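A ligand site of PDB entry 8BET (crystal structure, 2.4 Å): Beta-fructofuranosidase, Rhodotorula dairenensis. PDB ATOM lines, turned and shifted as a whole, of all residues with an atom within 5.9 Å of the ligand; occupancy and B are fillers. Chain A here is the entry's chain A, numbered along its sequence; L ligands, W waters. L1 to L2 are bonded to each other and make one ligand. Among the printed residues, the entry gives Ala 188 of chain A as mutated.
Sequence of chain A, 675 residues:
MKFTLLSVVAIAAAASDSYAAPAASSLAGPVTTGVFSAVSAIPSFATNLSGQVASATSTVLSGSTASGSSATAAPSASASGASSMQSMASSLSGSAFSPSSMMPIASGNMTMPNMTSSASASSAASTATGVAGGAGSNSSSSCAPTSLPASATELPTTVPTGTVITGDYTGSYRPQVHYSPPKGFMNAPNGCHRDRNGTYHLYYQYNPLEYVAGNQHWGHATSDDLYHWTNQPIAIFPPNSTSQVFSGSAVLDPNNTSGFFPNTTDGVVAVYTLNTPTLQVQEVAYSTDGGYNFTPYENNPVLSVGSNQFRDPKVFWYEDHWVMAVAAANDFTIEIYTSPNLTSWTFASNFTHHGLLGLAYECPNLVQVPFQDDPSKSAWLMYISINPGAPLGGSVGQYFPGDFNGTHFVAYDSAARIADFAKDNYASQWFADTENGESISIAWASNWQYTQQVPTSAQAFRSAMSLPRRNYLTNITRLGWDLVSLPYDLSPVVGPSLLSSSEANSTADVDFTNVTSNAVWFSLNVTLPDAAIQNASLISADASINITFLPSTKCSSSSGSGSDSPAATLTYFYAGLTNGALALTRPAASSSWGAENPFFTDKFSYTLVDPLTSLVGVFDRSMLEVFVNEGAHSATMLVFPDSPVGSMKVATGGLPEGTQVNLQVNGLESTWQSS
Water W3 lies within hydrogen-bond range of O3 of LIG L1 (2.7 Å), NE2 of Gln 280 (3.2 Å) and NH1 of Arg 311 (3.4 Å). Water W1 bridges O1 of LG2 L2 (2.7 Å) and NE1 of Trp 448 (3.1 Å). Water W4 lies within hydrogen-bond range of NE2 of Gln 216 (2.7 Å), O6 of LG2 L2 (2.8 Å) and OD1 of Asn 187 (3.0 Å). Water W2 bridges O of Asn 387 (2.8 Å) and O2 of LIG L1 (2.8 Å). Water W5 lies within hydrogen-bond range of NE2 of Gln 216 (3.0 Å) and O5 of LIG L1 (3.5 Å).
OE2 of Glu 362 is in hydrogen-bond range of O1 of LIG L1. The side-chain carboxylate (OD1) of Asp 312 lies within hydrogen-bond range of an oxygen (O4) of LG2 L2. An oxygen (O6) of LG2 L2 lies within hydrogen-bond range of the side-chain amide oxygen of Gln 205, at 2.7 Å. NE of Arg 311 is in hydrogen-bond range of O3 of LG2 L2, at 2.9 Å. The backbone NH (N) of Ser 247 lies within hydrogen-bond range of an oxygen (O4) of LG2 L2, at 2.9 Å. The side-chain hydroxyl (OG) of Ser 247 lies within hydrogen-bond range of an oxygen (O4) of LG2 L2, 3.1 Å away. ND2 of Asn 387 is in hydrogen-bond range of O1 of LIG L1, at 3.0 Å. An oxygen (O6) of LG2 L2 is in hydrogen-bond range of the side-chain amide nitrogen (ND2) of Asn 187, at 3.0 Å. An oxygen (O1) of LG2 L2 is in hydrogen-bond range of the side-chain sulfur (SG) of Cys 363, 3.6 Å away.
OE1 of Glu 362 lies within salt-bridge range of NH2 of Arg 311 (2.7 Å). The side-chain hydroxyl (OG1) of Thr 273 lies within hydrogen-bond range of the backbone NH (N) of Asp 312 (3.0 Å). O of Gln 205 is in hydrogen-bond range of N of Asn 187, at 2.9 Å. N of Gln 205 is in hydrogen-bond range of O of Ala 188 (2.9 Å). NE2 of Gln 205 lies within hydrogen-bond range of O of Val 245 (3.0 Å). The side-chain amide oxygen of Gln 280 lies within hydrogen-bond range of the guanidinium group of Arg 311 (3.0 Å). The backbone carbonyl oxygen (O) of Ser 247 is in hydrogen-bond range of the backbone NH (N) of Thr 273 (3.1 Å). The backbone NH (N) of Val 245 is in hydrogen-bond range of the backbone carbonyl oxygen (O) of Gln 216 (2.9 Å).
Ala 188 touches the ligand. Gln 216 touches the ligand. CB of Phe 246 touches O4 of LG2 L2, 3.6 Å away. Tyr 426 touches the ligand. CB of Ala 427 touches O1 of LG2 L2, at 3.99 Å. Trp 448 touches the ligand. Hydrophobic or aromatic side chains that line the ligand: Ala 188, Phe 246, Tyr 426, Ala 427 and Trp 448. 14 residues have an atom within 4 Å of the ligand: Asn 187, Ala 188, Gln 205, Gln 216, Phe 246, Ser 247, Arg 311, Asp 312, Glu 362, Cys 363, Asn 387, Tyr 426, Ala 427 and Trp 448. Along chain A the residues within 4 Å of the ligand span positions 187 to 448.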
ATOM      1  N   ASN A 187     -14.395 -22.721  27.687  1.00  0.00           N
ATOM      2  CA  ASN A 187     -15.662 -22.664  26.912  1.00  0.00           C
ATOM      3  C   ASN A 187     -15.347 -23.065  25.455  1.00  0.00           C
ATOM      4  O   ASN A 187     -14.784 -24.154  25.270  1.00  0.00           O
ATOM      5  CB  ASN A 187     -16.461 -21.380  27.190  1.00  0.00           C
ATOM      6  CG  ASN A 187     -15.735 -20.090  26.940  1.00  0.00           C
ATOM      7  OD1 ASN A 187     -14.850 -19.708  27.718  1.00  0.00           O
ATOM      8  ND2 ASN A 187     -16.149 -19.398  25.888  1.00  0.00           N
ATOM      9  N   ALA A 188     -15.679 -22.244  24.464  1.00  0.00           N
ATOM     10  CA  ALA A 188     -15.750 -22.627  23.028  1.00  0.00           C
ATOM     11  C   ALA A 188     -14.440 -23.236  22.534  1.00  0.00           C
ATOM     12  O   ALA A 188     -13.352 -22.776  22.876  1.00  0.00           O
ATOM     13  CB  ALA A 188     -16.140 -21.439  22.214  1.00  0.00           C
ATOM     14  N   GLN A 205     -11.280 -21.418  24.393  1.00  0.00           N
ATOM     15  CA  GLN A 205     -11.475 -20.258  25.286  1.00  0.00           C
ATOM     16  C   GLN A 205     -11.088 -20.699  26.706  1.00  0.00           C
ATOM     17  O   GLN A 205     -11.678 -21.694  27.202  1.00  0.00           O
ATOM     18  CB  GLN A 205     -12.905 -19.761  25.153  1.00  0.00           C
ATOM     19  CG  GLN A 205     -13.158 -19.084  23.815  1.00  0.00           C
ATOM     20  CD  GLN A 205     -12.405 -17.788  23.700  1.00  0.00           C
ATOM     21  OE1 GLN A 205     -12.821 -16.765  24.245  1.00  0.00           O
ATOM     22  NE2 GLN A 205     -11.280 -17.827  23.002  1.00  0.00           N
ATOM     23  N   ALA A 213     -16.018 -17.566  33.593  1.00  0.00           N
ATOM     24  CA  ALA A 213     -15.632 -16.913  32.327  1.00  0.00           C
ATOM     25  C   ALA A 213     -14.861 -15.627  32.639  1.00  0.00           C
ATOM     26  O   ALA A 213     -15.204 -14.976  33.635  1.00  0.00           O
ATOM     27  CB  ALA A 213     -16.872 -16.610  31.501  1.00  0.00           C
ATOM     28  N   GLN A 216      -9.902 -14.154  28.840  1.00  0.00           N
ATOM     29  CA  GLN A 216      -9.885 -15.203  27.798  1.00  0.00           C
ATOM     30  C   GLN A 216      -8.513 -15.253  27.117  1.00  0.00           C
ATOM     31  O   GLN A 216      -8.018 -14.241  26.645  1.00  0.00           O
ATOM     32  CB  GLN A 216     -11.048 -15.016  26.818  1.00  0.00           C
ATOM     33  CG  GLN A 216     -12.356 -15.560  27.386  1.00  0.00           C
ATOM     34  CD  GLN A 216     -13.146 -14.473  28.072  1.00  0.00           C
ATOM     35  OE1 GLN A 216     -12.628 -13.404  28.407  1.00  0.00           O
ATOM     36  NE2 GLN A 216     -14.420 -14.746  28.337  1.00  0.00           N
ATOM     37  N   VAL A 245      -8.690 -12.563  24.345  1.00  0.00           N
ATOM     38  CA  VAL A 245      -8.661 -13.313  23.062  1.00  0.00           C
ATOM     39  C   VAL A 245      -9.946 -14.143  22.972  1.00  0.00           C
ATOM     40  O   VAL A 245     -10.002 -15.192  23.604  1.00  0.00           O
ATOM     41  CB  VAL A 245      -7.415 -14.199  22.947  1.00  0.00           C
ATOM     42  CG1 VAL A 245      -7.306 -14.790  21.544  1.00  0.00           C
ATOM     43  CG2 VAL A 245      -6.135 -13.463  23.295  1.00  0.00           C
ATOM     44  N   PHE A 246     -10.938 -13.654  22.246  1.00  0.00           N
ATOM     45  CA  PHE A 246     -12.239 -14.317  22.008  1.00  0.00           C
ATOM     46  C   PHE A 246     -12.052 -15.351  20.898  1.00  0.00           C
ATOM     47  O   PHE A 246     -10.908 -15.611  20.468  1.00  0.00           O
ATOM     48  CB  PHE A 246     -13.340 -13.282  21.736  1.00  0.00           C
ATOM     49  CG  PHE A 246     -13.978 -12.680  22.967  1.00  0.00           C
ATOM     50  CD1 PHE A 246     -13.346 -12.721  24.204  1.00  0.00           C
ATOM     51  CD2 PHE A 246     -15.197 -12.046  22.900  1.00  0.00           C
ATOM     52  CE1 PHE A 246     -13.942 -12.173  25.337  1.00  0.00           C
ATOM     53  CE2 PHE A 246     -15.800 -11.505  24.028  1.00  0.00           C
ATOM     54  CZ  PHE A 246     -15.165 -11.565  25.243  1.00  0.00           C
ATOM     55  N   SER A 247     -13.139 -15.964  20.454  1.00  0.00           N
ATOM     56  CA  SER A 247     -13.086 -17.156  19.564  1.00  0.00           C
ATOM     57  C   SER A 247     -12.510 -16.791  18.202  1.00  0.00           C
ATOM     58  O   SER A 247     -12.512 -15.607  17.808  1.00  0.00           O
ATOM     59  CB  SER A 247     -14.415 -17.815  19.454  1.00  0.00           C
ATOM     60  OG  SER A 247     -14.752 -18.400  20.709  1.00  0.00           O
ATOM     61  N   GLY A 248     -12.041 -17.809  17.502  1.00  0.00           N
ATOM     62  CA  GLY A 248     -11.502 -17.699  16.148  1.00  0.00           C
ATOM     63  C   GLY A 248     -11.133 -19.049  15.592  1.00  0.00           C
ATOM     64  O   GLY A 248     -11.413 -20.059  16.249  1.00  0.00           O
ATOM     65  N   THR A 273     -11.116 -12.883  17.389  1.00  0.00           N
ATOM     66  CA  THR A 273     -11.664 -11.614  17.915  1.00  0.00           C
ATOM     67  C   THR A 273     -10.828 -11.191  19.121  1.00  0.00           C
ATOM     68  O   THR A 273     -10.635 -12.010  20.018  1.00  0.00           O
ATOM     69  CB  THR A 273     -13.146 -11.760  18.282  1.00  0.00           C
ATOM     70  OG1 THR A 273     -13.799 -12.213  17.099  1.00  0.00           O
ATOM     71  CG2 THR A 273     -13.750 -10.471  18.792  1.00  0.00           C
ATOM     72  N   GLN A 280     -14.993  -5.011  19.548  1.00  0.00           N
ATOM     73  CA  GLN A 280     -14.616  -6.374  19.113  1.00  0.00           C
ATOM     74  C   GLN A 280     -14.076  -6.246  17.688  1.00  0.00           C
ATOM     75  O   GLN A 280     -14.804  -5.770  16.816  1.00  0.00           O
ATOM     76  CB  GLN A 280     -15.814  -7.329  19.236  1.00  0.00           C
ATOM     77  CG  GLN A 280     -16.151  -7.666  20.685  1.00  0.00           C
ATOM     78  CD  GLN A 280     -17.282  -8.657  20.852  1.00  0.00           C
ATOM     79  OE1 GLN A 280     -18.024  -8.951  19.918  1.00  0.00           O
ATOM     80  NE2 GLN A 280     -17.402  -9.178  22.060  1.00  0.00           N
ATOM     81  N   GLN A 309     -19.997  -5.981  19.207  1.00  0.00           N
ATOM     82  CA  GLN A 309     -20.798  -7.208  18.973  1.00  0.00           C
ATOM     83  C   GLN A 309     -20.477  -7.704  17.554  1.00  0.00           C
ATOM     84  O   GLN A 309     -21.369  -7.650  16.661  1.00  0.00           O
ATOM     85  CB  GLN A 309     -22.289  -6.921  19.188  1.00  0.00           C
ATOM     86  CG  GLN A 309     -22.635  -6.388  20.569  1.00  0.00           C
ATOM     87  CD  GLN A 309     -22.335  -7.361  21.688  1.00  0.00           C
ATOM     88  OE1 GLN A 309     -22.109  -8.551  21.482  1.00  0.00           O
ATOM     89  NE2 GLN A 309     -22.328  -6.853  22.901  1.00  0.00           N
ATOM     90  N   ARG A 311     -17.798 -10.815  16.171  1.00  0.00           N
ATOM     91  CA  ARG A 311     -16.837 -11.833  16.673  1.00  0.00           C
ATOM     92  C   ARG A 311     -16.999 -13.222  16.043  1.00  0.00           C
ATOM     93  O   ARG A 311     -18.018 -13.478  15.350  1.00  0.00           O
ATOM     94  CB  ARG A 311     -16.990 -11.934  18.198  1.00  0.00           C
ATOM     95  CG  ARG A 311     -18.377 -12.313  18.669  1.00  0.00           C
ATOM     96  CD  ARG A 311     -18.393 -12.458  20.192  1.00  0.00           C
ATOM     97  NE  ARG A 311     -19.704 -12.750  20.722  1.00  0.00           N
ATOM     98  CZ  ARG A 311     -20.672 -11.861  20.947  1.00  0.00           C
ATOM     99  NH1 ARG A 311     -20.477 -10.588  20.684  1.00  0.00           N
ATOM    100  NH2 ARG A 311     -21.851 -12.272  21.408  1.00  0.00           N
ATOM    101  N   ASP A 312     -16.055 -14.118  16.347  1.00  0.00           N
ATOM    102  CA  ASP A 312     -16.079 -15.572  16.019  1.00  0.00           C
ATOM    103  C   ASP A 312     -15.801 -15.790  14.539  1.00  0.00           C
ATOM    104  O   ASP A 312     -16.584 -16.445  13.864  1.00  0.00           O
ATOM    105  CB  ASP A 312     -17.372 -16.211  16.542  1.00  0.00           C
ATOM    106  CG  ASP A 312     -17.664 -15.858  17.985  1.00  0.00           C
ATOM    107  OD1 ASP A 312     -16.721 -15.429  18.679  1.00  0.00           O
ATOM    108  OD2 ASP A 312     -18.839 -15.994  18.411  1.00  0.00           O
ATOM    109  N   TYR A 361     -26.365 -14.279  17.510  1.00  0.00           N
ATOM    110  CA  TYR A 361     -25.615 -15.204  16.624  1.00  0.00           C
ATOM    111  C   TYR A 361     -24.174 -15.259  17.114  1.00  0.00           C
ATOM    112  O   TYR A 361     -23.615 -14.199  17.399  1.00  0.00           O
ATOM    113  CB  TYR A 361     -25.638 -14.705  15.179  1.00  0.00           C
ATOM    114  CG  TYR A 361     -26.838 -15.075  14.343  1.00  0.00           C
ATOM    115  CD1 TYR A 361     -27.994 -15.612  14.882  1.00  0.00           C
ATOM    116  CD2 TYR A 361     -26.815 -14.812  12.984  1.00  0.00           C
ATOM    117  CE1 TYR A 361     -29.092 -15.902  14.080  1.00  0.00           C
ATOM    118  CE2 TYR A 361     -27.898 -15.096  12.175  1.00  0.00           C
ATOM    119  CZ  TYR A 361     -29.040 -15.650  12.718  1.00  0.00           C
ATOM    120  OH  TYR A 361     -30.055 -15.931  11.871  1.00  0.00           O
ATOM    121  N   GLU A 362     -23.602 -16.464  17.199  1.00  0.00           N
ATOM    122  CA  GLU A 362     -22.198 -16.688  17.620  1.00  0.00           C
ATOM    123  C   GLU A 362     -21.617 -17.861  16.838  1.00  0.00           C
ATOM    124  O   GLU A 362     -22.382 -18.662  16.302  1.00  0.00           O
ATOM    125  CB  GLU A 362     -22.131 -16.954  19.125  1.00  0.00           C
ATOM    126  CG  GLU A 362     -22.723 -15.829  19.947  1.00  0.00           C
ATOM    127  CD  GLU A 362     -22.489 -15.948  21.451  1.00  0.00           C
ATOM    128  OE1 GLU A 362     -22.397 -14.878  22.095  1.00  0.00           O
ATOM    129  OE2 GLU A 362     -22.439 -17.085  21.983  1.00  0.00           O
ATOM    130  N   CYS A 363     -20.288 -17.916  16.804  1.00  0.00           N
ATOM    131  CA  CYS A 363     -19.488 -19.086  16.360  1.00  0.00           C
ATOM    132  C   CYS A 363     -20.046 -19.646  15.052  1.00  0.00           C
ATOM    133  O   CYS A 363     -20.369 -20.828  14.985  1.00  0.00           O
ATOM    134  CB  CYS A 363     -19.460 -20.142  17.452  1.00  0.00           C
ATOM    135  SG  CYS A 363     -18.676 -19.498  18.947  1.00  0.00           S
ATOM    136  N   ASN A 387     -26.962 -17.726  21.789  1.00  0.00           N
ATOM    137  CA  ASN A 387     -26.908 -17.602  23.257  1.00  0.00           C
ATOM    138  C   ASN A 387     -27.035 -16.134  23.650  1.00  0.00           C
ATOM    139  O   ASN A 387     -26.427 -15.265  23.033  1.00  0.00           O
ATOM    140  CB  ASN A 387     -25.615 -18.155  23.857  1.00  0.00           C
ATOM    141  CG  ASN A 387     -25.624 -17.998  25.372  1.00  0.00           C
ATOM    142  OD1 ASN A 387     -26.469 -18.598  26.068  1.00  0.00           O
ATOM    143  ND2 ASN A 387     -24.707 -17.192  25.881  1.00  0.00           N
ATOM    144  N   PRO A 388     -27.834 -15.813  24.674  1.00  0.00           N
ATOM    145  CA  PRO A 388     -28.870 -16.727  25.188  1.00  0.00           C
ATOM    146  C   PRO A 388     -30.098 -16.853  24.296  1.00  0.00           C
ATOM    147  O   PRO A 388     -30.012 -16.453  23.177  1.00  0.00           O
ATOM    148  CB  PRO A 388     -29.252 -16.058  26.541  1.00  0.00           C
ATOM    149  CG  PRO A 388     -28.150 -15.059  26.819  1.00  0.00           C
ATOM    150  CD  PRO A 388     -27.741 -14.570  25.457  1.00  0.00           C
ATOM    151  N   TYR A 426     -22.821 -26.780  22.536  1.00  0.00           N
ATOM    152  CA  TYR A 426     -22.734 -25.388  22.052  1.00  0.00           C
ATOM    153  C   TYR A 426     -21.386 -25.124  21.392  1.00  0.00           C
ATOM    154  O   TYR A 426     -20.422 -25.798  21.714  1.00  0.00           O
ATOM    155  CB  TYR A 426     -22.940 -24.424  23.223  1.00  0.00           C
ATOM    156  CG  TYR A 426     -23.176 -22.991  22.815  1.00  0.00           C
ATOM    157  CD1 TYR A 426     -24.297 -22.656  22.067  1.00  0.00           C
ATOM    158  CD2 TYR A 426     -22.268 -21.999  23.118  1.00  0.00           C
ATOM    159  CE1 TYR A 426     -24.524 -21.355  21.675  1.00  0.00           C
ATOM    160  CE2 TYR A 426     -22.457 -20.692  22.709  1.00  0.00           C
ATOM    161  CZ  TYR A 426     -23.597 -20.366  22.000  1.00  0.00           C
ATOM    162  OH  TYR A 426     -23.833 -19.091  21.568  1.00  0.00           O
ATOM    163  N   ALA A 427     -21.362 -24.139  20.486  1.00  0.00           N
ATOM    164  CA  ALA A 427     -20.142 -23.572  19.877  1.00  0.00           C
ATOM    165  C   ALA A 427     -19.356 -24.684  19.163  1.00  0.00           C
ATOM    166  O   ALA A 427     -18.126 -24.657  19.226  1.00  0.00           O
ATOM    167  CB  ALA A 427     -19.323 -22.851  20.909  1.00  0.00           C
ATOM    168  N   TRP A 448     -24.700 -22.121  28.940  1.00  0.00           N
ATOM    169  CA  TRP A 448     -24.301 -20.843  29.586  1.00  0.00           C
ATOM    170  C   TRP A 448     -25.166 -20.518  30.817  1.00  0.00           C
ATOM    171  O   TRP A 448     -24.717 -19.711  31.630  1.00  0.00           O
ATOM    172  CB  TRP A 448     -24.291 -19.693  28.577  1.00  0.00           C
ATOM    173  CG  TRP A 448     -22.953 -19.592  27.913  1.00  0.00           C
ATOM    174  CD1 TRP A 448     -22.651 -19.881  26.615  1.00  0.00           C
ATOM    175  CD2 TRP A 448     -21.732 -19.199  28.543  1.00  0.00           C
ATOM    176  NE1 TRP A 448     -21.309 -19.684  26.405  1.00  0.00           N
ATOM    177  CE2 TRP A 448     -20.725 -19.240  27.565  1.00  0.00           C
ATOM    178  CE3 TRP A 448     -21.396 -18.783  29.838  1.00  0.00           C
ATOM    179  CZ2 TRP A 448     -19.397 -18.910  27.829  1.00  0.00           C
ATOM    180  CZ3 TRP A 448     -20.090 -18.430  30.101  1.00  0.00           C
ATOM    181  CH2 TRP A 448     -19.116 -18.508  29.110  1.00  0.00           C
HETATM  182  C1  LIG L   1     -19.813 -16.169  25.017  1.00  0.00           C
HETATM  183  C2  LIG L   1     -21.297 -15.933  25.320  1.00  0.00           C
HETATM  184  C3  LIG L   1     -21.667 -14.509  25.033  1.00  0.00           C
HETATM  185  C4  LIG L   1     -20.730 -13.537  25.712  1.00  0.00           C
HETATM  186  C5  LIG L   1     -19.267 -13.921  25.448  1.00  0.00           C
HETATM  187  C6  LIG L   1     -18.305 -13.009  26.175  1.00  0.00           C
HETATM  188  O1  LIG L   1     -22.091 -16.737  24.463  1.00  0.00           O
HETATM  189  O2  LIG L   1     -22.984 -14.223  25.475  1.00  0.00           O
HETATM  190  O3  LIG L   1     -21.039 -12.233  25.162  1.00  0.00           O
HETATM  191  O4  LIG L   1     -19.020 -15.301  25.807  1.00  0.00           O
HETATM  192  O5  LIG L   1     -18.680 -12.992  27.561  1.00  0.00           O
HETATM  193  C1  LG2 L   2     -19.634 -18.181  22.754  1.00  0.00           C
HETATM  194  C2  LG2 L   2     -18.804 -16.936  22.989  1.00  0.00           C
HETATM  195  C3  LG2 L   2     -18.270 -16.386  21.698  1.00  0.00           C
HETATM  196  C4  LG2 L   2     -16.996 -15.663  22.167  1.00  0.00           C
HETATM  197  C5  LG2 L   2     -16.519 -16.513  23.330  1.00  0.00           C
HETATM  198  C6  LG2 L   2     -15.965 -15.682  24.483  1.00  0.00           C
HETATM  199  O1  LG2 L   2     -18.733 -19.261  22.537  1.00  0.00           O
HETATM  200  O2  LG2 L   2     -19.558 -15.916  23.628  1.00  0.00           O
HETATM  201  O3  LG2 L   2     -19.252 -15.548  21.052  1.00  0.00           O
HETATM  202  O4  LG2 L   2     -15.969 -15.601  21.170  1.00  0.00           O
HETATM  203  O5  LG2 L   2     -17.653 -17.237  23.784  1.00  0.00           O
HETATM  204  O6  LG2 L   2     -15.259 -16.533  25.375  1.00  0.00           O
HETATM  205  O   HOH W   1     -19.089 -20.971  24.615  1.00  0.00           O
HETATM  206  O   HOH W   2     -24.970 -13.044  23.850  1.00  0.00           O
HETATM  207  O   HOH W   3     -19.709 -10.222  23.985  1.00  0.00           O
HETATM  208  O   HOH W   4     -15.982 -16.957  28.007  1.00  0.00           O
HETATM  209  O   HOH W   5     -16.274 -13.075  30.064  1.00  0.00           O
